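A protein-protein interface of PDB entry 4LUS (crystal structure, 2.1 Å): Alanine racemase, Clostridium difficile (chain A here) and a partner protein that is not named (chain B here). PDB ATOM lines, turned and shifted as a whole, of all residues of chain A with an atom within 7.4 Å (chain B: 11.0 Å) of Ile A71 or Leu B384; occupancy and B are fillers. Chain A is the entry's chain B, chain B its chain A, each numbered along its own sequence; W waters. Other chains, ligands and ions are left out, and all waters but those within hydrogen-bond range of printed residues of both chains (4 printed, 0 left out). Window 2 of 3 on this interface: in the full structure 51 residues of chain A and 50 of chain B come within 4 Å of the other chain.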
ATOM      1  N   VAL A  48      16.311  -7.781 -16.833  1.00  0.00           N
ATOM      2  CA  VAL A  48      17.475  -8.247 -16.125  1.00  0.00           C
ATOM      3  C   VAL A  48      17.397  -8.069 -14.606  1.00  0.00           C
ATOM      4  O   VAL A  48      17.687  -8.956 -13.897  1.00  0.00           O
ATOM      5  CB  VAL A  48      18.739  -7.600 -16.710  1.00  0.00           C
ATOM      6  CG1 VAL A  48      19.952  -7.703 -15.804  1.00  0.00           C
ATOM      7  CG2 VAL A  48      19.043  -8.167 -18.068  1.00  0.00           C
ATOM      8  N   VAL A  64      10.022 -15.373 -21.603  1.00  0.00           N
ATOM      9  CA  VAL A  64      10.353 -14.314 -22.510  1.00  0.00           C
ATOM     10  C   VAL A  64       9.620 -14.575 -23.803  1.00  0.00           C
ATOM     11  O   VAL A  64       9.017 -15.570 -23.939  1.00  0.00           O
ATOM     12  CB  VAL A  64      11.874 -14.089 -22.732  1.00  0.00           C
ATOM     13  CG1 VAL A  64      12.619 -13.940 -21.450  1.00  0.00           C
ATOM     14  CG2 VAL A  64      12.519 -15.121 -23.614  1.00  0.00           C
ATOM     15  N   ARG A  66      11.112 -13.424 -26.948  1.00  0.00           N
ATOM     16  CA  ARG A  66      12.106 -13.374 -27.992  1.00  0.00           C
ATOM     17  C   ARG A  66      13.418 -14.069 -27.597  1.00  0.00           C
ATOM     18  O   ARG A  66      13.782 -14.054 -26.477  1.00  0.00           O
ATOM     19  CB  ARG A  66      12.391 -11.916 -28.374  1.00  0.00           C
ATOM     20  CG  ARG A  66      11.220 -11.091 -28.880  1.00  0.00           C
ATOM     21  CD  ARG A  66      10.864 -11.335 -30.322  1.00  0.00           C
ATOM     22  NE  ARG A  66       9.771 -10.535 -30.811  1.00  0.00           N
ATOM     23  CZ  ARG A  66       8.518 -10.931 -30.828  1.00  0.00           C
ATOM     24  NH1 ARG A  66       8.208 -12.081 -30.346  1.00  0.00           N
ATOM     25  NH2 ARG A  66       7.587 -10.148 -31.268  1.00  0.00           N
ATOM     26  N   THR A  67      14.137 -14.606 -28.555  1.00  0.00           N
ATOM     27  CA  THR A  67      15.400 -15.236 -28.297  1.00  0.00           C
ATOM     28  C   THR A  67      16.391 -14.304 -27.653  1.00  0.00           C
ATOM     29  O   THR A  67      16.979 -14.631 -26.693  1.00  0.00           O
ATOM     30  CB  THR A  67      16.053 -15.739 -29.584  1.00  0.00           C
ATOM     31  OG1 THR A  67      15.162 -16.569 -30.300  1.00  0.00           O
ATOM     32  CG2 THR A  67      17.265 -16.502 -29.248  1.00  0.00           C
ATOM     33  N   ALA A  68      16.474 -13.098 -28.175  1.00  0.00           N
ATOM     34  CA  ALA A  68      17.336 -12.084 -27.635  1.00  0.00           C
ATOM     35  C   ALA A  68      17.057 -11.695 -26.210  1.00  0.00           C
ATOM     36  O   ALA A  68      17.957 -11.390 -25.513  1.00  0.00           O
ATOM     37  CB  ALA A  68      17.385 -10.884 -28.521  1.00  0.00           C
ATOM     38  N   GLU A  69      15.801 -11.701 -25.823  1.00  0.00           N
ATOM     39  CA  GLU A  69      15.415 -11.397 -24.487  1.00  0.00           C
ATOM     40  C   GLU A  69      16.011 -12.423 -23.545  1.00  0.00           C
ATOM     41  O   GLU A  69      16.489 -12.085 -22.525  1.00  0.00           O
ATOM     42  CB  GLU A  69      13.895 -11.298 -24.310  1.00  0.00           C
ATOM     43  CG  GLU A  69      13.258 -10.016 -24.777  1.00  0.00           C
ATOM     44  CD  GLU A  69      11.737 -10.005 -24.707  1.00  0.00           C
ATOM     45  OE1 GLU A  69      11.135 -11.015 -24.539  1.00  0.00           O
ATOM     46  OE2 GLU A  69      11.170  -8.963 -24.823  1.00  0.00           O
ATOM     47  N   GLY A  70      15.995 -13.677 -23.940  1.00  0.00           N
ATOM     48  CA  GLY A  70      16.712 -14.717 -23.250  1.00  0.00           C
ATOM     49  C   GLY A  70      18.221 -14.595 -23.206  1.00  0.00           C
ATOM     50  O   GLY A  70      18.781 -14.708 -22.186  1.00  0.00           O
ATOM     51  N   ILE A  71      18.843 -14.300 -24.316  1.00  0.00           N
ATOM     52  CA  ILE A  71      20.271 -14.115 -24.357  1.00  0.00           C
ATOM     53  C   ILE A  71      20.675 -12.974 -23.470  1.00  0.00           C
ATOM     54  O   ILE A  71      21.659 -13.037 -22.834  1.00  0.00           O
ATOM     55  CB  ILE A  71      20.782 -13.945 -25.782  1.00  0.00           C
ATOM     56  CG1 ILE A  71      20.381 -15.150 -26.614  1.00  0.00           C
ATOM     57  CG2 ILE A  71      22.274 -13.754 -25.826  1.00  0.00           C
ATOM     58  CD1 ILE A  71      20.882 -15.090 -27.999  1.00  0.00           C
ATOM     59  N   GLU A  72      19.842 -11.958 -23.395  1.00  0.00           N
ATOM     60  CA  GLU A  72      20.156 -10.803 -22.623  1.00  0.00           C
ATOM     61  C   GLU A  72      20.269 -11.236 -21.204  1.00  0.00           C
ATOM     62  O   GLU A  72      21.113 -10.817 -20.509  1.00  0.00           O
ATOM     63  CB  GLU A  72      19.110  -9.728 -22.791  1.00  0.00           C
ATOM     64  CG  GLU A  72      19.278  -8.560 -21.870  1.00  0.00           C
ATOM     65  CD  GLU A  72      18.093  -7.612 -21.872  1.00  0.00           C
ATOM     66  OE1 GLU A  72      17.026  -8.033 -22.222  1.00  0.00           O
ATOM     67  OE2 GLU A  72      18.252  -6.471 -21.504  1.00  0.00           O
ATOM     68  N   LEU A  73      19.386 -12.099 -20.795  1.00  0.00           N
ATOM     69  CA  LEU A  73      19.426 -12.669 -19.483  1.00  0.00           C
ATOM     70  C   LEU A  73      20.691 -13.514 -19.205  1.00  0.00           C
ATOM     71  O   LEU A  73      21.307 -13.342 -18.207  1.00  0.00           O
ATOM     72  CB  LEU A  73      18.130 -13.431 -19.176  1.00  0.00           C
ATOM     73  CG  LEU A  73      16.770 -12.712 -19.178  1.00  0.00           C
ATOM     74  CD1 LEU A  73      15.581 -13.639 -19.053  1.00  0.00           C
ATOM     75  CD2 LEU A  73      16.682 -11.588 -18.194  1.00  0.00           C
ATOM     76  N   ARG A  74      21.085 -14.366 -20.124  1.00  0.00           N
ATOM     77  CA  ARG A  74      22.281 -15.166 -19.959  1.00  0.00           C
ATOM     78  C   ARG A  74      23.529 -14.301 -19.850  1.00  0.00           C
ATOM     79  O   ARG A  74      24.377 -14.527 -19.068  1.00  0.00           O
ATOM     80  CB  ARG A  74      22.397 -16.163 -21.069  1.00  0.00           C
ATOM     81  CG  ARG A  74      21.317 -17.190 -21.126  1.00  0.00           C
ATOM     82  CD  ARG A  74      21.130 -17.949 -19.848  1.00  0.00           C
ATOM     83  NE  ARG A  74      20.148 -19.025 -19.940  1.00  0.00           N
ATOM     84  CZ  ARG A  74      19.494 -19.520 -18.917  1.00  0.00           C
ATOM     85  NH1 ARG A  74      19.725 -19.065 -17.730  1.00  0.00           N
ATOM     86  NH2 ARG A  74      18.639 -20.462 -19.092  1.00  0.00           N
ATOM     87  N   GLN A  75      23.551 -13.244 -20.620  1.00  0.00           N
ATOM     88  CA  GLN A  75      24.630 -12.314 -20.670  1.00  0.00           C
ATOM     89  C   GLN A  75      24.803 -11.566 -19.379  1.00  0.00           C
ATOM     90  O   GLN A  75      25.829 -11.024 -19.141  1.00  0.00           O
ATOM     91  CB  GLN A  75      24.518 -11.386 -21.882  1.00  0.00           C
ATOM     92  CG  GLN A  75      24.960 -12.016 -23.166  1.00  0.00           C
ATOM     93  CD  GLN A  75      24.966 -11.066 -24.325  1.00  0.00           C
ATOM     94  OE1 GLN A  75      24.680  -9.937 -24.188  1.00  0.00           O
ATOM     95  NE2 GLN A  75      25.277 -11.553 -25.462  1.00  0.00           N
ATOM     96  N   ASN A  76      23.762 -11.542 -18.576  1.00  0.00           N
ATOM     97  CA  ASN A  76      23.744 -10.859 -17.307  1.00  0.00           C
ATOM     98  C   ASN A  76      23.782 -11.795 -16.107  1.00  0.00           C
ATOM     99  O   ASN A  76      23.419 -11.451 -15.037  1.00  0.00           O
ATOM    100  CB  ASN A  76      22.601  -9.881 -17.214  1.00  0.00           C
ATOM    101  CG  ASN A  76      22.890  -8.582 -17.918  1.00  0.00           C
ATOM    102  OD1 ASN A  76      23.360  -7.674 -17.329  1.00  0.00           O
ATOM    103  ND2 ASN A  76      22.586  -8.521 -19.169  1.00  0.00           N
ATOM    104  N   GLY A  77      24.215 -13.000 -16.331  1.00  0.00           N
ATOM    105  CA  GLY A  77      24.315 -13.934 -15.258  1.00  0.00           C
ATOM    106  C   GLY A  77      23.110 -14.677 -14.760  1.00  0.00           C
ATOM    107  O   GLY A  77      23.212 -15.296 -13.777  1.00  0.00           O
ATOM    108  N   ILE A  82      14.781 -20.690 -18.742  1.00  0.00           N
ATOM    109  CA  ILE A  82      14.110 -19.673 -19.522  1.00  0.00           C
ATOM    110  C   ILE A  82      13.284 -20.269 -20.644  1.00  0.00           C
ATOM    111  O   ILE A  82      13.777 -20.982 -21.453  1.00  0.00           O
ATOM    112  CB  ILE A  82      15.094 -18.671 -20.169  1.00  0.00           C
ATOM    113  CG1 ILE A  82      15.886 -17.915 -19.144  1.00  0.00           C
ATOM    114  CG2 ILE A  82      14.411 -17.691 -21.069  1.00  0.00           C
ATOM    115  CD1 ILE A  82      16.964 -17.090 -19.738  1.00  0.00           C
ATOM    116  N   ALA A  92      17.696 -18.999 -35.426  1.00  0.00           N
ATOM    117  CA  ALA A  92      18.014 -18.764 -34.056  1.00  0.00           C
ATOM    118  C   ALA A  92      17.983 -20.024 -33.218  1.00  0.00           C
ATOM    119  O   ALA A  92      18.257 -19.962 -32.072  1.00  0.00           O
ATOM    120  CB  ALA A  92      17.130 -17.697 -33.484  1.00  0.00           C
ATOM    121  N   ASP A  95      21.488 -20.551 -31.380  1.00  0.00           N
ATOM    122  CA  ASP A  95      21.718 -19.609 -30.333  1.00  0.00           C
ATOM    123  C   ASP A  95      20.877 -19.941 -29.108  1.00  0.00           C
ATOM    124  O   ASP A  95      21.314 -19.764 -28.016  1.00  0.00           O
ATOM    125  CB  ASP A  95      21.504 -18.195 -30.783  1.00  0.00           C
ATOM    126  CG  ASP A  95      22.705 -17.610 -31.487  1.00  0.00           C
ATOM    127  OD1 ASP A  95      23.838 -18.034 -31.250  1.00  0.00           O
ATOM    128  OD2 ASP A  95      22.506 -16.705 -32.287  1.00  0.00           O
ATOM    129  N   SER A  96      19.677 -20.429 -29.340  1.00  0.00           N
ATOM    130  CA  SER A  96      18.835 -20.860 -28.293  1.00  0.00           C
ATOM    131  C   SER A  96      19.418 -22.017 -27.571  1.00  0.00           C
ATOM    132  O   SER A  96      19.459 -22.011 -26.392  1.00  0.00           O
ATOM    133  CB  SER A  96      17.492 -21.304 -28.839  1.00  0.00           C
ATOM    134  OG  SER A  96      16.730 -20.235 -29.282  1.00  0.00           O
ATOM    135  N   ASN A  99      22.439 -21.115 -25.507  1.00  0.00           N
ATOM    136  CA  ASN A  99      22.160 -20.280 -24.362  1.00  0.00           C
ATOM    137  C   ASN A  99      21.182 -20.909 -23.374  1.00  0.00           C
ATOM    138  O   ASN A  99      20.758 -20.286 -22.454  1.00  0.00           O
ATOM    139  CB  ASN A  99      21.731 -18.882 -24.762  1.00  0.00           C
ATOM    140  CG  ASN A  99      22.847 -18.070 -25.358  1.00  0.00           C
ATOM    141  OD1 ASN A  99      23.602 -17.440 -24.683  1.00  0.00           O
ATOM    142  ND2 ASN A  99      22.927 -18.089 -26.627  1.00  0.00           N
ATOM    143  N   ILE A 101      17.962 -21.889 -23.791  1.00  0.00           N
ATOM    144  CA  ILE A 101      16.634 -21.311 -23.810  1.00  0.00           C
ATOM    145  C   ILE A 101      15.632 -22.336 -24.272  1.00  0.00           C
ATOM    146  O   ILE A 101      15.706 -22.779 -25.354  1.00  0.00           O
ATOM    147  CB  ILE A 101      16.544 -20.148 -24.832  1.00  0.00           C
ATOM    148  CG1 ILE A 101      17.678 -19.163 -24.729  1.00  0.00           C
ATOM    149  CG2 ILE A 101      15.227 -19.446 -24.762  1.00  0.00           C
ATOM    150  CD1 ILE A 101      17.834 -18.589 -23.407  1.00  0.00           C
ATOM    151  N   LYS B   3      22.400 -13.441 -40.907  1.00  0.00           N
ATOM    152  CA  LYS B   3      23.081 -12.273 -40.369  1.00  0.00           C
ATOM    153  C   LYS B   3      22.181 -11.198 -39.692  1.00  0.00           C
ATOM    154  O   LYS B   3      22.434 -10.850 -38.594  1.00  0.00           O
ATOM    155  CB  LYS B   3      23.963 -11.653 -41.426  1.00  0.00           C
ATOM    156  CG  LYS B   3      24.803 -10.468 -41.029  1.00  0.00           C
ATOM    157  CD  LYS B   3      25.898 -10.790 -40.062  1.00  0.00           C
ATOM    158  CE  LYS B   3      26.661  -9.528 -39.744  1.00  0.00           C
ATOM    159  NZ  LYS B   3      27.375  -8.976 -40.930  1.00  0.00           N
ATOM    160  N   ILE B   4      20.880 -10.976 -39.868  1.00  0.00           N
ATOM    161  CA  ILE B   4      19.852 -10.482 -38.989  1.00  0.00           C
ATOM    162  C   ILE B   4      19.298 -11.659 -38.234  1.00  0.00           C
ATOM    163  O   ILE B   4      18.841 -12.550 -38.835  1.00  0.00           O
ATOM    164  CB  ILE B   4      18.700  -9.871 -39.797  1.00  0.00           C
ATOM    165  CG1 ILE B   4      19.128  -8.653 -40.571  1.00  0.00           C
ATOM    166  CG2 ILE B   4      17.570  -9.489 -38.910  1.00  0.00           C
ATOM    167  CD1 ILE B   4      18.011  -8.074 -41.360  1.00  0.00           C
ATOM    168  N   THR B   5      19.373 -11.677 -36.920  1.00  0.00           N
ATOM    169  CA  THR B   5      18.812 -12.771 -36.124  1.00  0.00           C
ATOM    170  C   THR B   5      17.490 -12.547 -35.395  1.00  0.00           C
ATOM    171  O   THR B   5      16.862 -13.479 -34.895  1.00  0.00           O
ATOM    172  CB  THR B   5      19.796 -13.237 -35.093  1.00  0.00           C
ATOM    173  OG1 THR B   5      20.322 -12.116 -34.429  1.00  0.00           O
ATOM    174  CG2 THR B   5      20.906 -13.961 -35.761  1.00  0.00           C
ATOM    175  N   VAL B   6      17.088 -11.302 -35.317  1.00  0.00           N
ATOM    176  CA  VAL B   6      15.834 -10.981 -34.746  1.00  0.00           C
ATOM    177  C   VAL B   6      14.677 -11.177 -35.699  1.00  0.00           C
ATOM    178  O   VAL B   6      14.822 -11.078 -36.865  1.00  0.00           O
ATOM    179  CB  VAL B   6      15.816  -9.578 -34.152  1.00  0.00           C
ATOM    180  CG1 VAL B   6      16.701  -9.504 -32.945  1.00  0.00           C
ATOM    181  CG2 VAL B   6      16.169  -8.551 -35.171  1.00  0.00           C
ATOM    182  N   PRO B   7      13.522 -11.519 -35.184  1.00  0.00           N
ATOM    183  CA  PRO B   7      12.326 -11.618 -35.998  1.00  0.00           C
ATOM    184  C   PRO B   7      11.768 -10.285 -36.535  1.00  0.00           C
ATOM    185  O   PRO B   7      11.043 -10.335 -37.474  1.00  0.00           O
ATOM    186  CB  PRO B   7      11.356 -12.288 -35.082  1.00  0.00           C
ATOM    187  CG  PRO B   7      11.762 -11.860 -33.774  1.00  0.00           C
ATOM    188  CD  PRO B   7      13.198 -11.577 -33.770  1.00  0.00           C
ATOM    189  N   ARG B 364      12.993  -0.795 -27.862  1.00  0.00           N
ATOM    190  CA  ARG B 364      14.357  -1.135 -27.602  1.00  0.00           C
ATOM    191  C   ARG B 364      14.708  -2.485 -28.202  1.00  0.00           C
ATOM    192  O   ARG B 364      15.746  -2.628 -28.694  1.00  0.00           O
ATOM    193  CB  ARG B 364      14.710  -1.108 -26.108  1.00  0.00           C
ATOM    194  CG  ARG B 364      16.192  -1.234 -25.806  1.00  0.00           C
ATOM    195  CD  ARG B 364      16.667  -1.066 -24.357  1.00  0.00           C
ATOM    196  NE  ARG B 364      16.047  -2.121 -23.702  1.00  0.00           N
ATOM    197  CZ  ARG B 364      16.581  -3.164 -23.160  1.00  0.00           C
ATOM    198  NH1 ARG B 364      17.845  -3.319 -23.002  1.00  0.00           N
ATOM    199  NH2 ARG B 364      15.763  -4.030 -22.720  1.00  0.00           N
ATOM    200  N   ARG B 365      13.794  -3.429 -28.166  1.00  0.00           N
ATOM    201  CA  ARG B 365      14.055  -4.746 -28.703  1.00  0.00           C
ATOM    202  C   ARG B 365      14.091  -4.848 -30.217  1.00  0.00           C
ATOM    203  O   ARG B 365      14.464  -5.821 -30.736  1.00  0.00           O
ATOM    204  CB  ARG B 365      13.187  -5.827 -28.073  1.00  0.00           C
ATOM    205  CG  ARG B 365      11.733  -5.878 -28.440  1.00  0.00           C
ATOM    206  CD  ARG B 365      11.001  -7.031 -27.797  1.00  0.00           C
ATOM    207  NE  ARG B 365       9.655  -7.146 -28.296  1.00  0.00           N
ATOM    208  CZ  ARG B 365       8.685  -7.845 -27.756  1.00  0.00           C
ATOM    209  NH1 ARG B 365       8.872  -8.530 -26.662  1.00  0.00           N
ATOM    210  NH2 ARG B 365       7.514  -7.835 -28.325  1.00  0.00           N
ATOM    211  N   VAL B 366      13.671  -3.807 -30.886  1.00  0.00           N
ATOM    212  CA  VAL B 366      13.695  -3.790 -32.322  1.00  0.00           C
ATOM    213  C   VAL B 366      15.088  -3.292 -32.812  1.00  0.00           C
ATOM    214  O   VAL B 366      15.397  -2.157 -32.725  1.00  0.00           O
ATOM    215  CB  VAL B 366      12.564  -2.904 -32.868  1.00  0.00           C
ATOM    216  CG1 VAL B 366      12.614  -2.804 -34.352  1.00  0.00           C
ATOM    217  CG2 VAL B 366      11.220  -3.336 -32.374  1.00  0.00           C
ATOM    218  N   ASP B 367      15.902  -4.206 -33.306  1.00  0.00           N
ATOM    219  CA  ASP B 367      17.249  -3.946 -33.773  1.00  0.00           C
ATOM    220  C   ASP B 367      17.240  -2.992 -34.940  1.00  0.00           C
ATOM    221  O   ASP B 367      16.431  -3.081 -35.791  1.00  0.00           O
ATOM    222  CB  ASP B 367      17.939  -5.199 -34.292  1.00  0.00           C
ATOM    223  CG  ASP B 367      18.333  -6.179 -33.221  1.00  0.00           C
ATOM    224  OD1 ASP B 367      18.084  -6.029 -32.071  1.00  0.00           O
ATOM    225  OD2 ASP B 367      18.915  -7.136 -33.569  1.00  0.00           O
ATOM    226  N   ARG B 368      18.186  -2.085 -34.947  1.00  0.00           N
ATOM    227  CA  ARG B 368      18.379  -1.164 -36.030  1.00  0.00           C
ATOM    228  C   ARG B 368      19.435  -1.717 -36.985  1.00  0.00           C
ATOM    229  O   ARG B 368      20.521  -1.942 -36.610  1.00  0.00           O
ATOM    230  CB  ARG B 368      18.760   0.207 -35.501  1.00  0.00           C
ATOM    231  CG  ARG B 368      17.601   1.130 -35.221  1.00  0.00           C
ATOM    232  CD  ARG B 368      16.642   0.582 -34.217  1.00  0.00           C
ATOM    233  NE  ARG B 368      15.738   1.576 -33.783  1.00  0.00           N
ATOM    234  CZ  ARG B 368      14.883   1.461 -32.790  1.00  0.00           C
ATOM    235  NH1 ARG B 368      14.789   0.392 -32.112  1.00  0.00           N
ATOM    236  NH2 ARG B 368      14.120   2.453 -32.502  1.00  0.00           N
ATOM    237  N   GLN B 378      25.858  -2.476 -40.864  1.00  0.00           N
ATOM    238  CA  GLN B 378      25.828  -2.533 -39.421  1.00  0.00           C
ATOM    239  C   GLN B 378      24.483  -2.945 -38.834  1.00  0.00           C
ATOM    240  O   GLN B 378      23.473  -2.478 -39.264  1.00  0.00           O
ATOM    241  CB  GLN B 378      26.229  -1.168 -38.900  1.00  0.00           C
ATOM    242  CG  GLN B 378      26.033  -0.948 -37.446  1.00  0.00           C
ATOM    243  CD  GLN B 378      27.295  -0.584 -36.748  1.00  0.00           C
ATOM    244  OE1 GLN B 378      28.325  -0.428 -37.355  1.00  0.00           O
ATOM    245  NE2 GLN B 378      27.217  -0.465 -35.461  1.00  0.00           N
ATOM    246  N   ILE B 379      24.527  -3.752 -37.802  1.00  0.00           N
ATOM    247  CA  ILE B 379      23.403  -4.118 -36.968  1.00  0.00           C
ATOM    248  C   ILE B 379      23.612  -3.719 -35.510  1.00  0.00           C
ATOM    249  O   ILE B 379      24.530  -4.133 -34.893  1.00  0.00           O
ATOM    250  CB  ILE B 379      23.145  -5.642 -36.953  1.00  0.00           C
ATOM    251  CG1 ILE B 379      22.983  -6.199 -38.330  1.00  0.00           C
ATOM    252  CG2 ILE B 379      21.950  -5.959 -36.112  1.00  0.00           C
ATOM    253  CD1 ILE B 379      22.473  -7.592 -38.388  1.00  0.00           C
ATOM    254  N   ASN B 380      22.693  -2.964 -34.968  1.00  0.00           N
ATOM    255  CA  ASN B 380      22.698  -2.616 -33.563  1.00  0.00           C
ATOM    256  C   ASN B 380      21.600  -3.297 -32.758  1.00  0.00           C
ATOM    257  O   ASN B 380      20.457  -3.214 -33.067  1.00  0.00           O
ATOM    258  CB  ASN B 380      22.624  -1.111 -33.358  1.00  0.00           C
ATOM    259  CG  ASN B 380      23.825  -0.378 -33.882  1.00  0.00           C
ATOM    260  OD1 ASN B 380      24.817  -0.949 -34.177  1.00  0.00           O
ATOM    261  ND2 ASN B 380      23.701   0.887 -34.020  1.00  0.00           N
ATOM    262  N   SER B 381      21.997  -3.979 -31.728  1.00  0.00           N
ATOM    263  CA  SER B 381      21.083  -4.524 -30.783  1.00  0.00           C
ATOM    264  C   SER B 381      21.163  -3.670 -29.559  1.00  0.00           C
ATOM    265  O   SER B 381      22.219  -3.389 -29.069  1.00  0.00           O
ATOM    266  CB  SER B 381      21.383  -5.959 -30.417  1.00  0.00           C
ATOM    267  OG  SER B 381      20.671  -6.316 -29.293  1.00  0.00           O
ATOM    268  N   TYR B 382      20.020  -3.251 -29.095  1.00  0.00           N
ATOM    269  CA  TYR B 382      19.962  -2.542 -27.883  1.00  0.00           C
ATOM    270  C   TYR B 382      19.903  -3.470 -26.690  1.00  0.00           C
ATOM    271  O   TYR B 382      20.008  -3.043 -25.609  1.00  0.00           O
ATOM    272  CB  TYR B 382      18.830  -1.524 -27.880  1.00  0.00           C
ATOM    273  CG  TYR B 382      19.008  -0.344 -28.788  1.00  0.00           C
ATOM    274  CD1 TYR B 382      20.260   0.120 -29.137  1.00  0.00           C
ATOM    275  CD2 TYR B 382      17.924   0.305 -29.299  1.00  0.00           C
ATOM    276  CE1 TYR B 382      20.403   1.191 -29.978  1.00  0.00           C
ATOM    277  CE2 TYR B 382      18.056   1.376 -30.114  1.00  0.00           C
ATOM    278  CZ  TYR B 382      19.295   1.830 -30.464  1.00  0.00           C
ATOM    279  OH  TYR B 382      19.390   2.887 -31.277  1.00  0.00           O
ATOM    280  N   LEU B 383      19.745  -4.746 -26.926  1.00  0.00           N
ATOM    281  CA  LEU B 383      19.699  -5.710 -25.857  1.00  0.00           C
ATOM    282  C   LEU B 383      21.009  -6.441 -25.553  1.00  0.00           C
ATOM    283  O   LEU B 383      21.269  -6.749 -24.465  1.00  0.00           O
ATOM    284  CB  LEU B 383      18.587  -6.707 -26.108  1.00  0.00           C
ATOM    285  CG  LEU B 383      17.227  -6.371 -25.547  1.00  0.00           C
ATOM    286  CD1 LEU B 383      16.732  -5.046 -26.056  1.00  0.00           C
ATOM    287  CD2 LEU B 383      16.217  -7.451 -25.780  1.00  0.00           C
ATOM    288  N   LEU B 384      21.802  -6.697 -26.559  1.00  0.00           N
ATOM    289  CA  LEU B 384      22.947  -7.557 -26.423  1.00  0.00           C
ATOM    290  C   LEU B 384      24.324  -6.901 -26.430  1.00  0.00           C
ATOM    291  O   LEU B 384      24.521  -5.864 -26.945  1.00  0.00           O
ATOM    292  CB  LEU B 384      22.905  -8.719 -27.386  1.00  0.00           C
ATOM    293  CG  LEU B 384      21.626  -9.505 -27.486  1.00  0.00           C
ATOM    294  CD1 LEU B 384      21.575 -10.444 -28.643  1.00  0.00           C
ATOM    295  CD2 LEU B 384      21.081 -10.106 -26.224  1.00  0.00           C
HETATM  296  O   HOH W   1      14.753  -6.413 -22.314  1.00  0.00           O
HETATM  297  O   HOH W   2      14.855 -14.930 -32.789  1.00  0.00           O
HETATM  298  O   HOH W   3      20.738  -5.361 -22.181  1.00  0.00           O
HETATM  299  O   HOH W   4      22.907  -8.281 -22.851  1.00  0.00           O
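Of the 20 printed residues of chain A, 6 touch a printed residue of chain B.
Hydrophobic or aromatic side chains of chain A within 4 Å of the printed part of chain B: Ile A71.
Of the 17 printed residues of chain B, 5 touch a printed residue of chain A.
Printed residues of chain B that touch a printed residue of chain A: Pro B7, Arg B364, Arg B365, Leu B383 and Leu B384.
Among the printed residues, 9 pairs touch across the chains.
OE1 of Glu A69 sits at hydrogen-bond distance from N of Arg A66 (3.4 Å).
ND2 of Asn A76 lies within hydrogen-bond range of O of Glu A72.
The guanidinium group (NH1) of Arg B364 lies within hydrogen-bond range of the backbone carbonyl oxygen (O) of Tyr B382, at 3.4 Å.
The side-chain hydroxyl of Ser B381 lies within hydrogen-bond range of the backbone NH of Leu B384 (3.0 Å).
The side-chain hydroxyl (OG) of Ser B381 is in hydrogen-bond range of the backbone NH (N) of Leu B383 (3.0 Å).
CG of Pro B7 touches CD of Arg A66 (3.6 Å).
NH2 of Arg A66 touches NH2 of Arg B365, at 3.7 Å.
CD2 of Leu B384 touches O of Ala A68, 3.5 Å away.
Leu B384 touches Ile A71 (CD2 to CG2, 3.9 Å).
CD2 of Leu B383 touches OE1 of Glu A72, 3.7 Å away.
Glu A72 touches Leu B384.
Gln A75 touches Leu B384.
Thr A67 touches none of the printed residues of chain B.
Ala A68 touches one residue of chain B.
No residue of chain B comes within 4 Å of Gly A70.
Leu A73 touches none of the printed residues of chain B.
Arg A74 touches none of the printed residues of chain B.
Of the printed residues of chain A, Pro B7 touches Arg A66 (3.6 Å).
Of the printed residues of chain A, Arg B364 touches Glu A72 (3.5 Å).
Printed residues of chain A within 4 Å of Arg B365: Arg A66 and Glu A69.
Of the printed residues of chain A, Leu B383 touches Glu A72 (3.7 Å).
Printed residues of chain A within 4 Å of Leu B384: Ala A68 (3.5 Å), Ile A71 (3.9 Å), Glu A72 (3.6 Å) and Gln A75 (3.7 Å).
The nearest residue of chain B that does not touch Ile A71 is Leu B383 (6.3 Å).
The nearest residue of chain A that does not touch Leu B384 is Glu A69 (5.5 Å).
The nearest printed residue of chain B that does not touch Arg A66 is Leu B383 (6.4 Å).
Water W1 bridges the guanidinium group of Arg B364 and the side-chain carboxylate of Glu A72.
Water W3 bridges O of Leu B383 and OE2 of Glu A72.
Water W4 lies within hydrogen-bond range of the backbone carbonyl oxygen (O) of Leu B383 (2.8 Å) and the side-chain amide oxygen (OE1) of Gln A75 (2.8 Å).
Water W2 lies within hydrogen-bond range of OG1 of Thr A67 and O of Thr B5.
NH1 of Arg B365 lies within salt-bridge range of OE2 of Glu A69, at 3.0 Å.
NH1 of Arg B364 is in salt-bridge range of OE2 of Glu A72, at 3.5 Å.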
